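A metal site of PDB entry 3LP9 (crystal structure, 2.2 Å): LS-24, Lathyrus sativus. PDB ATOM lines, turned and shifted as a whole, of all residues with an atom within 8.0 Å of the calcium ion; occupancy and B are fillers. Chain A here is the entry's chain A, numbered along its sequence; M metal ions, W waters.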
ATOM      1  N   THR A   1     -16.186  21.804  23.269  1.00  0.00           N
ATOM      2  CA  THR A   1     -17.092  20.762  23.810  1.00  0.00           C
ATOM      3  C   THR A   1     -16.636  20.225  25.174  1.00  0.00           C
ATOM      4  O   THR A   1     -15.497  19.908  25.343  1.00  0.00           O
ATOM      5  CB  THR A   1     -17.220  19.534  22.857  1.00  0.00           C
ATOM      6  OG1 THR A   1     -17.514  19.978  21.547  1.00  0.00           O
ATOM      7  CG2 THR A   1     -18.357  18.586  23.362  1.00  0.00           C
ATOM      8  N   TYR A   5     -20.634  15.490  25.979  1.00  0.00           N
ATOM      9  CA  TYR A   5     -21.526  16.127  25.002  1.00  0.00           C
ATOM     10  C   TYR A   5     -21.131  15.835  23.582  1.00  0.00           C
ATOM     11  O   TYR A   5     -19.982  15.423  23.317  1.00  0.00           O
ATOM     12  CB  TYR A   5     -21.693  17.619  25.227  1.00  0.00           C
ATOM     13  CG  TYR A   5     -22.440  17.923  26.528  1.00  0.00           C
ATOM     14  CD1 TYR A   5     -23.852  17.846  26.605  1.00  0.00           C
ATOM     15  CD2 TYR A   5     -21.739  18.320  27.650  1.00  0.00           C
ATOM     16  CE1 TYR A   5     -24.513  18.127  27.819  1.00  0.00           C
ATOM     17  CE2 TYR A   5     -22.389  18.544  28.893  1.00  0.00           C
ATOM     18  CZ  TYR A   5     -23.754  18.448  28.961  1.00  0.00           C
ATOM     19  OH  TYR A   5     -24.316  18.695  30.169  1.00  0.00           O
ATOM     20  N   ILE A   6     -22.058  16.012  22.663  1.00  0.00           N
ATOM     21  CA  ILE A   6     -21.824  15.756  21.254  1.00  0.00           C
ATOM     22  C   ILE A   6     -20.722  16.643  20.732  1.00  0.00           C
ATOM     23  O   ILE A   6     -20.832  17.842  20.761  1.00  0.00           O
ATOM     24  CB  ILE A   6     -23.082  15.968  20.377  1.00  0.00           C
ATOM     25  CG1 ILE A   6     -24.283  15.204  20.932  1.00  0.00           C
ATOM     26  CG2 ILE A   6     -22.822  15.454  19.030  1.00  0.00           C
ATOM     27  CD1 ILE A   6     -25.563  15.456  20.168  1.00  0.00           C
ATOM     28  N   ASN A   7     -19.667  16.013  20.230  1.00  0.00           N
ATOM     29  CA  ASN A   7     -18.502  16.701  19.730  1.00  0.00           C
ATOM     30  C   ASN A   7     -18.384  16.652  18.227  1.00  0.00           C
ATOM     31  O   ASN A   7     -17.638  17.437  17.661  1.00  0.00           O
ATOM     32  CB  ASN A   7     -17.255  16.095  20.407  1.00  0.00           C
ATOM     33  CG  ASN A   7     -16.019  16.951  20.296  1.00  0.00           C
ATOM     34  OD1 ASN A   7     -16.075  18.181  20.112  1.00  0.00           O
ATOM     35  ND2 ASN A   7     -14.887  16.313  20.452  1.00  0.00           N
ATOM     36  N   ALA A   8     -19.127  15.759  17.561  1.00  0.00           N
ATOM     37  CA  ALA A   8     -19.126  15.651  16.119  1.00  0.00           C
ATOM     38  C   ALA A   8     -20.411  14.964  15.655  1.00  0.00           C
ATOM     39  O   ALA A   8     -21.007  14.261  16.431  1.00  0.00           O
ATOM     40  CB  ALA A   8     -17.896  14.899  15.620  1.00  0.00           C
ATOM     41  N   ALA A   9     -20.839  15.160  14.396  1.00  0.00           N
ATOM     42  CA  ALA A   9     -21.983  14.492  13.871  1.00  0.00           C
ATOM     43  C   ALA A   9     -21.922  14.502  12.364  1.00  0.00           C
ATOM     44  O   ALA A   9     -21.428  15.437  11.770  1.00  0.00           O
ATOM     45  CB  ALA A   9     -23.276  15.187  14.328  1.00  0.00           C
ATOM     46  N   PHE A  21     -20.757  11.805  17.648  1.00  0.00           N
ATOM     47  CA  PHE A  21     -19.523  11.448  18.312  1.00  0.00           C
ATOM     48  C   PHE A  21     -19.377  12.170  19.647  1.00  0.00           C
ATOM     49  O   PHE A  21     -19.452  13.392  19.710  1.00  0.00           O
ATOM     50  CB  PHE A  21     -18.319  11.639  17.377  1.00  0.00           C
ATOM     51  CG  PHE A  21     -18.423  10.864  16.098  1.00  0.00           C
ATOM     52  CD1 PHE A  21     -18.131   9.506  16.079  1.00  0.00           C
ATOM     53  CD2 PHE A  21     -18.895  11.466  14.957  1.00  0.00           C
ATOM     54  CE1 PHE A  21     -18.309   8.760  14.921  1.00  0.00           C
ATOM     55  CE2 PHE A  21     -19.076  10.737  13.784  1.00  0.00           C
ATOM     56  CZ  PHE A  21     -18.777   9.355  13.764  1.00  0.00           C
ATOM     57  N   ILE A  64     -13.385  11.328  17.755  1.00  0.00           N
ATOM     58  CA  ILE A  64     -13.499  12.210  16.588  1.00  0.00           C
ATOM     59  C   ILE A  64     -14.142  13.513  17.030  1.00  0.00           C
ATOM     60  O   ILE A  64     -15.208  13.475  17.661  1.00  0.00           O
ATOM     61  CB  ILE A  64     -14.411  11.543  15.481  1.00  0.00           C
ATOM     62  CG1 ILE A  64     -13.729  10.290  14.906  1.00  0.00           C
ATOM     63  CG2 ILE A  64     -14.870  12.571  14.363  1.00  0.00           C
ATOM     64  CD1 ILE A  64     -14.560   9.480  13.985  1.00  0.00           C
ATOM     65  N   ASP A  65     -13.550  14.659  16.691  1.00  0.00           N
ATOM     66  CA  ASP A  65     -14.116  15.945  17.185  1.00  0.00           C
ATOM     67  C   ASP A  65     -14.798  16.842  16.189  1.00  0.00           C
ATOM     68  O   ASP A  65     -15.402  17.796  16.572  1.00  0.00           O
ATOM     69  CB  ASP A  65     -13.063  16.699  17.958  1.00  0.00           C
ATOM     70  CG  ASP A  65     -11.900  17.114  17.096  1.00  0.00           C
ATOM     71  OD1 ASP A  65     -12.107  17.374  15.841  1.00  0.00           O
ATOM     72  OD2 ASP A  65     -10.812  17.286  17.700  1.00  0.00           O
ATOM     73  N   CYS A  66     -14.744  16.533  14.903  1.00  0.00           N
ATOM     74  CA  CYS A  66     -15.480  17.231  13.891  1.00  0.00           C
ATOM     75  C   CYS A  66     -15.615  16.230  12.714  1.00  0.00           C
ATOM     76  O   CYS A  66     -14.838  15.256  12.625  1.00  0.00           O
ATOM     77  CB  CYS A  66     -14.781  18.527  13.456  1.00  0.00           C
ATOM     78  SG  CYS A  66     -15.700  19.526  12.195  1.00  0.00           S
ATOM     79  N   SER A  67     -16.628  16.455  11.870  1.00  0.00           N
ATOM     80  CA  SER A  67     -16.925  15.591  10.725  1.00  0.00           C
ATOM     81  C   SER A  67     -17.949  16.157   9.796  1.00  0.00           C
ATOM     82  O   SER A  67     -18.555  17.155  10.086  1.00  0.00           O
ATOM     83  CB  SER A  67     -17.431  14.208  11.175  1.00  0.00           C
ATOM     84  OG  SER A  67     -18.667  14.283  11.853  1.00  0.00           O
ATOM     85  N   PHE A  78     -12.186  14.458  11.928  1.00  0.00           N
ATOM     86  CA  PHE A  78     -11.054  15.313  12.401  1.00  0.00           C
ATOM     87  C   PHE A  78     -10.819  14.936  13.867  1.00  0.00           C
ATOM     88  O   PHE A  78     -11.737  14.481  14.550  1.00  0.00           O
ATOM     89  CB  PHE A  78     -11.427  16.800  12.273  1.00  0.00           C
ATOM     90  CG  PHE A  78     -11.693  17.272  10.867  1.00  0.00           C
ATOM     91  CD1 PHE A  78     -10.788  18.026  10.215  1.00  0.00           C
ATOM     92  CD2 PHE A  78     -12.904  16.979  10.231  1.00  0.00           C
ATOM     93  CE1 PHE A  78     -11.012  18.496   8.876  1.00  0.00           C
ATOM     94  CE2 PHE A  78     -13.206  17.476   8.901  1.00  0.00           C
ATOM     95  CZ  PHE A  78     -12.206  18.217   8.219  1.00  0.00           C
ATOM     96  N   ILE A 120     -11.079  22.066  13.999  1.00  0.00           N
ATOM     97  CA  ILE A 120     -12.378  22.547  13.583  1.00  0.00           C
ATOM     98  C   ILE A 120     -13.420  22.107  14.606  1.00  0.00           C
ATOM     99  O   ILE A 120     -13.336  21.007  15.162  1.00  0.00           O
ATOM    100  CB  ILE A 120     -12.633  22.019  12.181  1.00  0.00           C
ATOM    101  CG1 ILE A 120     -11.454  22.398  11.287  1.00  0.00           C
ATOM    102  CG2 ILE A 120     -13.990  22.553  11.657  1.00  0.00           C
ATOM    103  CD1 ILE A 120     -11.754  22.130   9.863  1.00  0.00           C
ATOM    104  N   ASP A 121     -14.344  22.995  14.940  1.00  0.00           N
ATOM    105  CA  ASP A 121     -15.404  22.688  15.913  1.00  0.00           C
ATOM    106  C   ASP A 121     -16.541  21.849  15.281  1.00  0.00           C
ATOM    107  O   ASP A 121     -16.881  20.751  15.766  1.00  0.00           O
ATOM    108  CB  ASP A 121     -15.972  23.971  16.506  1.00  0.00           C
ATOM    109  CG  ASP A 121     -15.003  24.717  17.420  1.00  0.00           C
ATOM    110  OD1 ASP A 121     -14.028  24.132  17.896  1.00  0.00           O
ATOM    111  OD2 ASP A 121     -15.220  25.897  17.724  1.00  0.00           O
ATOM    112  N   ALA A 122     -17.087  22.356  14.183  1.00  0.00           N
ATOM    113  CA  ALA A 122     -18.230  21.727  13.609  1.00  0.00           C
ATOM    114  C   ALA A 122     -18.311  21.964  12.089  1.00  0.00           C
ATOM    115  O   ALA A 122     -17.636  22.866  11.581  1.00  0.00           O
ATOM    116  CB  ALA A 122     -19.505  22.307  14.279  1.00  0.00           C
ATOM    117  N   ALA A 123     -19.197  21.224  11.403  1.00  0.00           N
ATOM    118  CA  ALA A 123     -19.316  21.247   9.957  1.00  0.00           C
ATOM    119  C   ALA A 123     -20.564  20.527   9.526  1.00  0.00           C
ATOM    120  O   ALA A 123     -21.001  19.616  10.194  1.00  0.00           O
ATOM    121  CB  ALA A 123     -18.143  20.576   9.307  1.00  0.00           C
ATOM    122  N   PHE A 135     -16.991  25.411  11.059  1.00  0.00           N
ATOM    123  CA  PHE A 135     -16.992  26.378  12.155  1.00  0.00           C
ATOM    124  C   PHE A 135     -15.822  26.181  13.083  1.00  0.00           C
ATOM    125  O   PHE A 135     -15.514  25.060  13.452  1.00  0.00           O
ATOM    126  CB  PHE A 135     -18.326  26.287  12.966  1.00  0.00           C
ATOM    127  CG  PHE A 135     -19.558  26.561  12.109  1.00  0.00           C
ATOM    128  CD1 PHE A 135     -20.129  27.832  12.050  1.00  0.00           C
ATOM    129  CD2 PHE A 135     -20.111  25.542  11.297  1.00  0.00           C
ATOM    130  CE1 PHE A 135     -21.230  28.072  11.257  1.00  0.00           C
ATOM    131  CE2 PHE A 135     -21.220  25.759  10.452  1.00  0.00           C
ATOM    132  CZ  PHE A 135     -21.778  27.033  10.435  1.00  0.00           C
ATOM    133  N   ALA A 174     -20.124  26.448  17.776  1.00  0.00           N
ATOM    134  CA  ALA A 174     -20.880  25.222  17.999  1.00  0.00           C
ATOM    135  C   ALA A 174     -20.004  24.013  18.398  1.00  0.00           C
ATOM    136  O   ALA A 174     -18.840  23.902  18.047  1.00  0.00           O
ATOM    137  CB  ALA A 174     -21.706  24.919  16.736  1.00  0.00           C
ATOM    138  N   ASP A 175     -20.593  23.120  19.180  1.00  0.00           N
ATOM    139  CA  ASP A 175     -19.953  21.882  19.582  1.00  0.00           C
ATOM    140  C   ASP A 175     -19.873  20.904  18.371  1.00  0.00           C
ATOM    141  O   ASP A 175     -18.827  20.316  18.090  1.00  0.00           O
ATOM    142  CB  ASP A 175     -20.699  21.246  20.759  1.00  0.00           C
ATOM    143  CG  ASP A 175     -20.342  21.866  22.108  1.00  0.00           C
ATOM    144  OD1 ASP A 175     -19.480  22.792  22.121  1.00  0.00           O
ATOM    145  OD2 ASP A 175     -20.917  21.440  23.131  1.00  0.00           O
ATOM    146  N   ALA A 176     -20.989  20.765  17.665  1.00  0.00           N
ATOM    147  CA  ALA A 176     -21.128  19.855  16.539  1.00  0.00           C
ATOM    148  C   ALA A 176     -22.317  20.297  15.643  1.00  0.00           C
ATOM    149  O   ALA A 176     -23.133  21.173  16.024  1.00  0.00           O
ATOM    150  CB  ALA A 176     -21.382  18.488  17.010  1.00  0.00           C
ATOM    151  N   ALA A 177     -22.448  19.633  14.497  1.00  0.00           N
ATOM    152  CA  ALA A 177     -23.541  19.904  13.582  1.00  0.00           C
ATOM    153  C   ALA A 177     -23.685  18.806  12.555  1.00  0.00           C
ATOM    154  O   ALA A 177     -22.813  17.960  12.441  1.00  0.00           O
ATOM    155  CB  ALA A 177     -23.350  21.248  12.916  1.00  0.00           C
ATOM    156  N   PHE A 189     -25.367  21.756  17.617  1.00  0.00           N
ATOM    157  CA  PHE A 189     -25.367  21.378  19.041  1.00  0.00           C
ATOM    158  C   PHE A 189     -24.350  22.237  19.790  1.00  0.00           C
ATOM    159  O   PHE A 189     -23.334  22.693  19.217  1.00  0.00           O
ATOM    160  CB  PHE A 189     -24.998  19.893  19.227  1.00  0.00           C
ATOM    161  CG  PHE A 189     -25.871  18.920  18.448  1.00  0.00           C
ATOM    162  CD1 PHE A 189     -27.237  18.749  18.752  1.00  0.00           C
ATOM    163  CD2 PHE A 189     -25.327  18.168  17.408  1.00  0.00           C
ATOM    164  CE1 PHE A 189     -28.027  17.852  18.040  1.00  0.00           C
ATOM    165  CE2 PHE A 189     -26.107  17.244  16.671  1.00  0.00           C
ATOM    166  CZ  PHE A 189     -27.481  17.082  17.014  1.00  0.00           C
HETATM  167 CA    CA M   1     -16.406  19.581  17.948  1.00  0.00          CA
HETATM  168  O   HOH W   1     -13.557  20.099  17.978  1.00  0.00           O
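O of Phe 78 sits at hydrogen-bond distance from N of Asp 65 (2.8 Å). N of Asn 7 lies within hydrogen-bond range of O of Phe 21. The backbone NH (N) of Asp 175 is in hydrogen-bond range of the backbone carbonyl oxygen (O) of Phe 189, 2.8 Å away. N of Asp 121 sits at hydrogen-bond distance from O of Phe 135. The side-chain carboxylate (OD1) of Asp 175 lies close to the side-chain hydroxyl (OG1) of Thr 1 (3.5 Å). The side-chain hydroxyl (OG1) of Thr 1 lies close to the side-chain amide oxygen (OD1) of Asn 7, 2.7 Å away.
OG1 of Thr 1 touches the calcium ion (3.8 Å). Of the 22 residues printed, 5 come within 4 Å of the calcium ion.
The calcium ion is bound by O of Asp 65 (2.5 Å), O of Asn 7 (2.5 Å), O of Asp 121 (2.5 Å), O of Asp 175 (2.5 Å), OD1 of Asn 7 (2.6 Å) and water W1 (2.9 Å). The calcium ion has six donor atoms within binding distance.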
